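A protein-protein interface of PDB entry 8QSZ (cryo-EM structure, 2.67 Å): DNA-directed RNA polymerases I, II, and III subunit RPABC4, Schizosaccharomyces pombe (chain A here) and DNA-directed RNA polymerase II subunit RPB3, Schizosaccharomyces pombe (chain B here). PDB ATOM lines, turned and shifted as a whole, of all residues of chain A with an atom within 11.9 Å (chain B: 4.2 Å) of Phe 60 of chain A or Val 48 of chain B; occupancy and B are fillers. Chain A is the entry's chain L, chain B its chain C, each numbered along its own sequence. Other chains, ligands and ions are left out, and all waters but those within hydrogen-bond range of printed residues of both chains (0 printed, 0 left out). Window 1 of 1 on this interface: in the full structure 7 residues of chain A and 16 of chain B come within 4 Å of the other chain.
The backbone carbonyl oxygen of Val 58 of chain A lies within hydrogen-bond range of the backbone NH of Ile 50 of chain B, 2.9 Å away. The backbone NH (N) of Val 48 of chain B sits at hydrogen-bond distance from the backbone carbonyl oxygen (O) of Phe 60 of chain A (2.5 Å). The backbone carbonyl oxygen (O) of Asp 46 of chain B is in hydrogen-bond range of the backbone NH (N) of Ala 62 of chain A (2.5 Å). The side-chain carboxylate (OE2) of Glu 49 of chain B is in hydrogen-bond range of the side-chain amide nitrogen (NE2) of Gln 59 of chain A (2.7 Å). The guanidinium group (NH2) of Arg 63 of chain A is in salt-bridge range of the side-chain carboxylate (OD1) of Asp 46 of chain B, at 3.3 Å. The guanidinium group (NH2) of Arg 53 of chain A is in salt-bridge range of the side-chain carboxylate (OD1) of Asp 59 of chain B (3.7 Å).
The guanidinium group (NE) of Arg 63 of chain A is in salt-bridge range of the side-chain carboxylate (OE1) of Glu 61 of chain A (2.9 Å). N of Glu 49 of chain B lies within hydrogen-bond range of O of Arg 157 of chain B (2.9 Å).
Among the printed residues, pairs that only touch across the chains: Ala 62 of chain A with Ala 63 of chain B (3.0 Å), Glu 61 of chain A with Asp 46 of chain B (3.0 Å), Gln 59 of chain A with Val 48 of chain B (3.1 Å), Val 58 of chain A with Glu 49 of chain B (3.2 Å), Ala 62 of chain A with Ile 45 of chain B (3.3 Å), Phe 60 of chain A with Asp 59 of chain B (3.3 Å), Phe 60 of chain A with Leu 47 of chain B (3.5 Å), Gln 59 of chain A with Leu 47 of chain B (3.7 Å), Val 58 of chain A with Asp 59 of chain B (3.7 Å), Phe 60 of chain A with Ile 50 of chain B (3.7 Å), Val 58 of chain A with Val 48 of chain B (3.8 Å), Phe 60 of chain A with Ala 63 of chain B (3.8 Å), Phe 60 of chain A with Asp 46 of chain B (3.8 Å), Arg 53 of chain A with Ile 50 of chain B (3.9 Å) and Glu 61 of chain A with Leu 47 of chain B (3.98 Å).
Of the printed residues of chain B, Arg 53 of chain A touches Ile 50 and Asp 59. Of the printed residues of chain B, Val 58 of chain A touches Val 48, Glu 49, Ile 50 and Asp 59. Phe 60 of chain A touches just these residues of chain B: Asp 46, Leu 47, Val 48, Ile 50, Asp 59 and Ala 63. Of the printed residues of chain B, Glu 61 of chain A touches Asp 46 (3.0 Å) and Leu 47 (3.98 Å). Of the printed residues of chain B, Ala 62 of chain A touches Ile 45, Asp 46 and Ala 63. Of the printed residues of chain B, Arg 63 of chain A touches Asp 46 (3.3 Å). Of chain A, only Ala 62 comes within 4 Å of Ile 45 of chain B. Glu 49 of chain B touches two residues of chain A. Of chain A, only Arg 53 (3.9 Å), Val 58 (2.9 Å) and Phe 60 (3.7 Å) come within 4 Å of Ile 50 of chain B. Of chain A, only Arg 53 (2.3 Å), Val 58 (3.7 Å) and Phe 60 (3.3 Å) come within 4 Å of Asp 59 of chain B. No residue of chain A comes within 4 Å of Glu 60 of chain B. Ala 63 of chain B touches two residues of chain A.
Of the 10 printed residues of chain B, 8 touch a printed residue of chain A. Hydrophobic or aromatic side chains of chain B within 4 Å of the printed part of chain A: Leu 47, Val 48, Ile 50 and Ala 63. Hydrophobic or aromatic side chains of chain A that line the printed part of chain B: Val 58, Phe 60 and Ala 62. Among the printed residues, Asp or Glu carboxylates within 4 Å of a Lys or Arg side-chain nitrogen of the other chain: Arg 53 of chain A with Asp 59 of chain B (2.3 Å) and Arg 63 of chain A with Asp 46 of chain B (3.3 Å).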
ATOM      1  N   ARG A  53     -42.017  -2.277  31.555  1.00  0.00           N
ATOM      2  CA  ARG A  53     -40.746  -2.286  30.850  1.00  0.00           C
ATOM      3  C   ARG A  53     -40.084  -3.649  30.960  1.00  0.00           C
ATOM      4  O   ARG A  53     -40.028  -4.244  32.037  1.00  0.00           O
ATOM      5  CB  ARG A  53     -39.828  -1.210  31.422  1.00  0.00           C
ATOM      6  CG  ARG A  53     -38.868  -0.636  30.419  1.00  0.00           C
ATOM      7  CD  ARG A  53     -37.622  -0.110  31.088  1.00  0.00           C
ATOM      8  NE  ARG A  53     -36.628   0.281  30.099  1.00  0.00           N
ATOM      9  CZ  ARG A  53     -36.628   1.440  29.456  1.00  0.00           C
ATOM     10  NH1 ARG A  53     -37.549   2.360  29.686  1.00  0.00           N
ATOM     11  NH2 ARG A  53     -35.683   1.677  28.554  1.00  0.00           N
ATOM     12  N   THR A  54     -39.577  -4.138  29.832  1.00  0.00           N
ATOM     13  CA  THR A  54     -38.948  -5.448  29.799  1.00  0.00           C
ATOM     14  C   THR A  54     -37.802  -5.522  30.804  1.00  0.00           C
ATOM     15  O   THR A  54     -37.279  -4.509  31.273  1.00  0.00           O
ATOM     16  CB  THR A  54     -38.428  -5.757  28.395  1.00  0.00           C
ATOM     17  OG1 THR A  54     -38.018  -7.124  28.327  1.00  0.00           O
ATOM     18  CG2 THR A  54     -37.250  -4.865  28.050  1.00  0.00           C
ATOM     19  N   ARG A  56     -35.029  -7.169  29.914  1.00  0.00           N
ATOM     20  CA  ARG A  56     -33.825  -7.256  29.106  1.00  0.00           C
ATOM     21  C   ARG A  56     -32.949  -6.024  29.302  1.00  0.00           C
ATOM     22  O   ARG A  56     -33.385  -4.981  29.792  1.00  0.00           O
ATOM     23  CB  ARG A  56     -34.183  -7.408  27.630  1.00  0.00           C
ATOM     24  CG  ARG A  56     -34.833  -8.728  27.297  1.00  0.00           C
ATOM     25  CD  ARG A  56     -35.176  -8.837  25.828  1.00  0.00           C
ATOM     26  NE  ARG A  56     -35.773 -10.132  25.524  1.00  0.00           N
ATOM     27  CZ  ARG A  56     -37.071 -10.393  25.561  1.00  0.00           C
ATOM     28  NH1 ARG A  56     -37.957  -9.465  25.888  1.00  0.00           N
ATOM     29  NH2 ARG A  56     -37.493 -11.621  25.276  1.00  0.00           N
ATOM     30  N   MET A  57     -31.685  -6.169  28.920  1.00  0.00           N
ATOM     31  CA  MET A  57     -30.744  -5.067  29.023  1.00  0.00           C
ATOM     32  C   MET A  57     -31.026  -4.043  27.935  1.00  0.00           C
ATOM     33  O   MET A  57     -31.285  -4.391  26.780  1.00  0.00           O
ATOM     34  CB  MET A  57     -29.310  -5.581  28.903  1.00  0.00           C
ATOM     35  CG  MET A  57     -28.961  -6.713  29.859  1.00  0.00           C
ATOM     36  SD  MET A  57     -28.497  -6.141  31.502  1.00  0.00           S
ATOM     37  CE  MET A  57     -30.072  -6.238  32.352  1.00  0.00           C
ATOM     38  N   VAL A  58     -30.979  -2.769  28.309  1.00  0.00           N
ATOM     39  CA  VAL A  58     -31.247  -1.664  27.400  1.00  0.00           C
ATOM     40  C   VAL A  58     -29.998  -0.804  27.345  1.00  0.00           C
ATOM     41  O   VAL A  58     -29.619  -0.194  28.351  1.00  0.00           O
ATOM     42  CB  VAL A  58     -32.460  -0.831  27.849  1.00  0.00           C
ATOM     43  CG1 VAL A  58     -32.443   0.531  27.191  1.00  0.00           C
ATOM     44  CG2 VAL A  58     -33.753  -1.561  27.538  1.00  0.00           C
ATOM     45  N   GLN A  59     -29.361  -0.751  26.182  1.00  0.00           N
ATOM     46  CA  GLN A  59     -28.156   0.041  25.991  1.00  0.00           C
ATOM     47  C   GLN A  59     -28.333   0.955  24.793  1.00  0.00           C
ATOM     48  O   GLN A  59     -28.737   0.511  23.716  1.00  0.00           O
ATOM     49  CB  GLN A  59     -26.936  -0.855  25.786  1.00  0.00           C
ATOM     50  CG  GLN A  59     -25.622  -0.107  25.726  1.00  0.00           C
ATOM     51  CD  GLN A  59     -24.524  -0.937  25.116  1.00  0.00           C
ATOM     52  OE1 GLN A  59     -24.662  -1.445  24.006  1.00  0.00           O
ATOM     53  NE2 GLN A  59     -23.427  -1.090  25.843  1.00  0.00           N
ATOM     54  N   PHE A  60     -28.032   2.236  24.988  1.00  0.00           N
ATOM     55  CA  PHE A  60     -28.066   3.229  23.926  1.00  0.00           C
ATOM     56  C   PHE A  60     -26.745   3.970  23.877  1.00  0.00           C
ATOM     57  O   PHE A  60     -26.218   4.387  24.911  1.00  0.00           O
ATOM     58  CB  PHE A  60     -29.206   4.230  24.126  1.00  0.00           C
ATOM     59  CG  PHE A  60     -30.564   3.639  23.936  1.00  0.00           C
ATOM     60  CD1 PHE A  60     -31.058   3.420  22.666  1.00  0.00           C
ATOM     61  CD2 PHE A  60     -31.344   3.298  25.019  1.00  0.00           C
ATOM     62  CE1 PHE A  60     -32.298   2.871  22.482  1.00  0.00           C
ATOM     63  CE2 PHE A  60     -32.584   2.749  24.837  1.00  0.00           C
ATOM     64  CZ  PHE A  60     -33.063   2.538  23.568  1.00  0.00           C
ATOM     65  N   GLU A  61     -26.210   4.134  22.674  1.00  0.00           N
ATOM     66  CA  GLU A  61     -25.028   4.958  22.490  1.00  0.00           C
ATOM     67  C   GLU A  61     -25.451   6.409  22.323  1.00  0.00           C
ATOM     68  O   GLU A  61     -26.463   6.708  21.689  1.00  0.00           O
ATOM     69  CB  GLU A  61     -24.216   4.473  21.291  1.00  0.00           C
ATOM     70  CG  GLU A  61     -24.922   4.568  19.962  1.00  0.00           C
ATOM     71  CD  GLU A  61     -23.955   4.547  18.801  1.00  0.00           C
ATOM     72  OE1 GLU A  61     -22.734   4.482  19.049  1.00  0.00           O
ATOM     73  OE2 GLU A  61     -24.413   4.603  17.640  1.00  0.00           O
ATOM     74  N   ALA A  62     -24.666   7.314  22.897  1.00  0.00           N
ATOM     75  CA  ALA A  62     -25.092   8.696  23.093  1.00  0.00           C
ATOM     76  C   ALA A  62     -24.720   9.584  21.924  1.00  0.00           C
ATOM     77  O   ALA A  62     -24.462  10.778  22.090  1.00  0.00           O
ATOM     78  CB  ALA A  62     -24.496   9.231  24.388  1.00  0.00           C
ATOM     79  N   ARG A  63     -24.672   9.017  20.726  1.00  0.00           N
ATOM     80  CA  ARG A  63     -24.330   9.772  19.537  1.00  0.00           C
ATOM     81  C   ARG A  63     -25.544   9.911  18.629  1.00  0.00           C
ATOM     82  O   ARG A  63     -26.423  10.737  18.876  1.00  0.00           O
ATOM     83  CB  ARG A  63     -23.181   9.095  18.799  1.00  0.00           C
ATOM     84  CG  ARG A  63     -23.458   7.684  18.391  1.00  0.00           C
ATOM     85  CD  ARG A  63     -22.262   7.094  17.684  1.00  0.00           C
ATOM     86  NE  ARG A  63     -21.155   6.864  18.602  1.00  0.00           N
ATOM     87  CZ  ARG A  63     -19.907   6.629  18.224  1.00  0.00           C
ATOM     88  NH1 ARG A  63     -19.562   6.619  16.948  1.00  0.00           N
ATOM     89  NH2 ARG A  63     -18.983   6.397  19.149  1.00  0.00           N
ATOM     90  N   ILE B  45     -19.736  11.002  27.394  1.00  0.00           N
ATOM     91  CA  ILE B  45     -20.589   9.844  27.614  1.00  0.00           C
ATOM     92  C   ILE B  45     -20.913   9.204  26.273  1.00  0.00           C
ATOM     93  O   ILE B  45     -21.403   9.865  25.350  1.00  0.00           O
ATOM     94  CB  ILE B  45     -21.868  10.250  28.367  1.00  0.00           C
ATOM     95  CG1 ILE B  45     -21.575  10.445  29.853  1.00  0.00           C
ATOM     96  CG2 ILE B  45     -22.949   9.205  28.188  1.00  0.00           C
ATOM     97  CD1 ILE B  45     -22.507  11.416  30.534  1.00  0.00           C
ATOM     98  N   ASP B  46     -20.628   7.907  26.154  1.00  0.00           N
ATOM     99  CA  ASP B  46     -20.835   7.195  24.896  1.00  0.00           C
ATOM    100  C   ASP B  46     -21.931   6.148  25.029  1.00  0.00           C
ATOM    101  O   ASP B  46     -22.910   6.210  24.284  1.00  0.00           O
ATOM    102  CB  ASP B  46     -19.526   6.568  24.419  1.00  0.00           C
ATOM    103  CG  ASP B  46     -19.544   6.239  22.939  1.00  0.00           C
ATOM    104  OD1 ASP B  46     -20.297   6.888  22.187  1.00  0.00           O
ATOM    105  OD2 ASP B  46     -18.804   5.328  22.526  1.00  0.00           O
ATOM    106  N   LEU B  47     -21.817   5.201  25.957  1.00  0.00           N
ATOM    107  CA  LEU B  47     -22.785   4.112  26.068  1.00  0.00           C
ATOM    108  C   LEU B  47     -23.662   4.329  27.293  1.00  0.00           C
ATOM    109  O   LEU B  47     -23.153   4.536  28.391  1.00  0.00           O
ATOM    110  CB  LEU B  47     -22.081   2.760  26.161  1.00  0.00           C
ATOM    111  CG  LEU B  47     -21.190   2.353  24.991  1.00  0.00           C
ATOM    112  CD1 LEU B  47     -20.494   1.052  25.309  1.00  0.00           C
ATOM    113  CD2 LEU B  47     -21.992   2.226  23.715  1.00  0.00           C
ATOM    114  N   VAL B  48     -24.975   4.272  27.114  1.00  0.00           N
ATOM    115  CA  VAL B  48     -25.918   4.467  28.207  1.00  0.00           C
ATOM    116  C   VAL B  48     -26.705   3.178  28.395  1.00  0.00           C
ATOM    117  O   VAL B  48     -27.348   2.693  27.457  1.00  0.00           O
ATOM    118  CB  VAL B  48     -26.851   5.655  27.943  1.00  0.00           C
ATOM    119  CG1 VAL B  48     -27.761   5.882  29.125  1.00  0.00           C
ATOM    120  CG2 VAL B  48     -26.040   6.900  27.654  1.00  0.00           C
ATOM    121  N   GLU B  49     -26.650   2.622  29.604  1.00  0.00           N
ATOM    122  CA  GLU B  49     -27.446   1.466  29.990  1.00  0.00           C
ATOM    123  C   GLU B  49     -28.558   1.949  30.910  1.00  0.00           C
ATOM    124  O   GLU B  49     -28.285   2.476  31.992  1.00  0.00           O
ATOM    125  CB  GLU B  49     -26.589   0.416  30.695  1.00  0.00           C
ATOM    126  CG  GLU B  49     -25.270   0.094  30.006  1.00  0.00           C
ATOM    127  CD  GLU B  49     -25.352  -1.113  29.097  1.00  0.00           C
ATOM    128  OE1 GLU B  49     -26.372  -1.832  29.135  1.00  0.00           O
ATOM    129  OE2 GLU B  49     -24.387  -1.345  28.337  1.00  0.00           O
ATOM    130  N   ILE B  50     -29.803   1.756  30.490  1.00  0.00           N
ATOM    131  CA  ILE B  50     -30.960   2.332  31.163  1.00  0.00           C
ATOM    132  C   ILE B  50     -31.710   1.214  31.869  1.00  0.00           C
ATOM    133  O   ILE B  50     -32.135   0.241  31.234  1.00  0.00           O
ATOM    134  CB  ILE B  50     -31.866   3.078  30.172  1.00  0.00           C
ATOM    135  CG1 ILE B  50     -31.130   4.298  29.617  1.00  0.00           C
ATOM    136  CG2 ILE B  50     -33.158   3.498  30.843  1.00  0.00           C
ATOM    137  CD1 ILE B  50     -31.751   4.890  28.388  1.00  0.00           C
ATOM    138  N   ASP B  59     -35.794   7.254  25.511  1.00  0.00           N
ATOM    139  CA  ASP B  59     -34.501   6.773  25.985  1.00  0.00           C
ATOM    140  C   ASP B  59     -33.356   7.329  25.150  1.00  0.00           C
ATOM    141  O   ASP B  59     -32.349   7.794  25.696  1.00  0.00           O
ATOM    142  CB  ASP B  59     -34.471   5.249  25.966  1.00  0.00           C
ATOM    143  CG  ASP B  59     -34.992   4.643  27.243  1.00  0.00           C
ATOM    144  OD1 ASP B  59     -35.666   5.353  28.017  1.00  0.00           O
ATOM    145  OD2 ASP B  59     -34.727   3.447  27.470  1.00  0.00           O
ATOM    146  N   GLU B  60     -33.476   7.274  23.822  1.00  0.00           N
ATOM    147  CA  GLU B  60     -32.384   7.745  22.978  1.00  0.00           C
ATOM    148  C   GLU B  60     -32.310   9.266  22.958  1.00  0.00           C
ATOM    149  O   GLU B  60     -31.228   9.826  22.767  1.00  0.00           O
ATOM    150  CB  GLU B  60     -32.528   7.175  21.568  1.00  0.00           C
ATOM    151  CG  GLU B  60     -33.672   7.738  20.754  1.00  0.00           C
ATOM    152  CD  GLU B  60     -34.990   7.056  21.039  1.00  0.00           C
ATOM    153  OE1 GLU B  60     -35.051   6.242  21.981  1.00  0.00           O
ATOM    154  OE2 GLU B  60     -35.969   7.344  20.323  1.00  0.00           O
ATOM    155  N   ALA B  63     -30.188   9.692  25.959  1.00  0.00           N
ATOM    156  CA  ALA B  63     -28.822   9.279  25.669  1.00  0.00           C
ATOM    157  C   ALA B  63     -28.090  10.344  24.868  1.00  0.00           C
ATOM    158  O   ALA B  63     -26.955  10.713  25.188  1.00  0.00           O
ATOM    159  CB  ALA B  63     -28.832   7.951  24.910  1.00  0.00           C
ATOM    160  N   ARG B 157     -26.751   4.090  33.842  1.00  0.00           N
ATOM    161  CA  ARG B 157     -25.302   4.046  33.972  1.00  0.00           C
ATOM    162  C   ARG B 157     -24.670   4.425  32.641  1.00  0.00           C
ATOM    163  O   ARG B 157     -24.992   3.832  31.608  1.00  0.00           O
ATOM    164  CB  ARG B 157     -24.843   2.651  34.391  1.00  0.00           C
ATOM    165  CG  ARG B 157     -23.463   2.608  35.002  1.00  0.00           C
ATOM    166  CD  ARG B 157     -23.185   1.251  35.637  1.00  0.00           C
ATOM    167  NE  ARG B 157     -23.546   0.113  34.797  1.00  0.00           N
ATOM    168  CZ  ARG B 157     -23.178  -0.065  33.534  1.00  0.00           C
ATOM    169  NH1 ARG B 157     -22.321   0.745  32.936  1.00  0.00           N
ATOM    170  NH2 ARG B 157     -23.666  -1.101  32.858  1.00  0.00           N
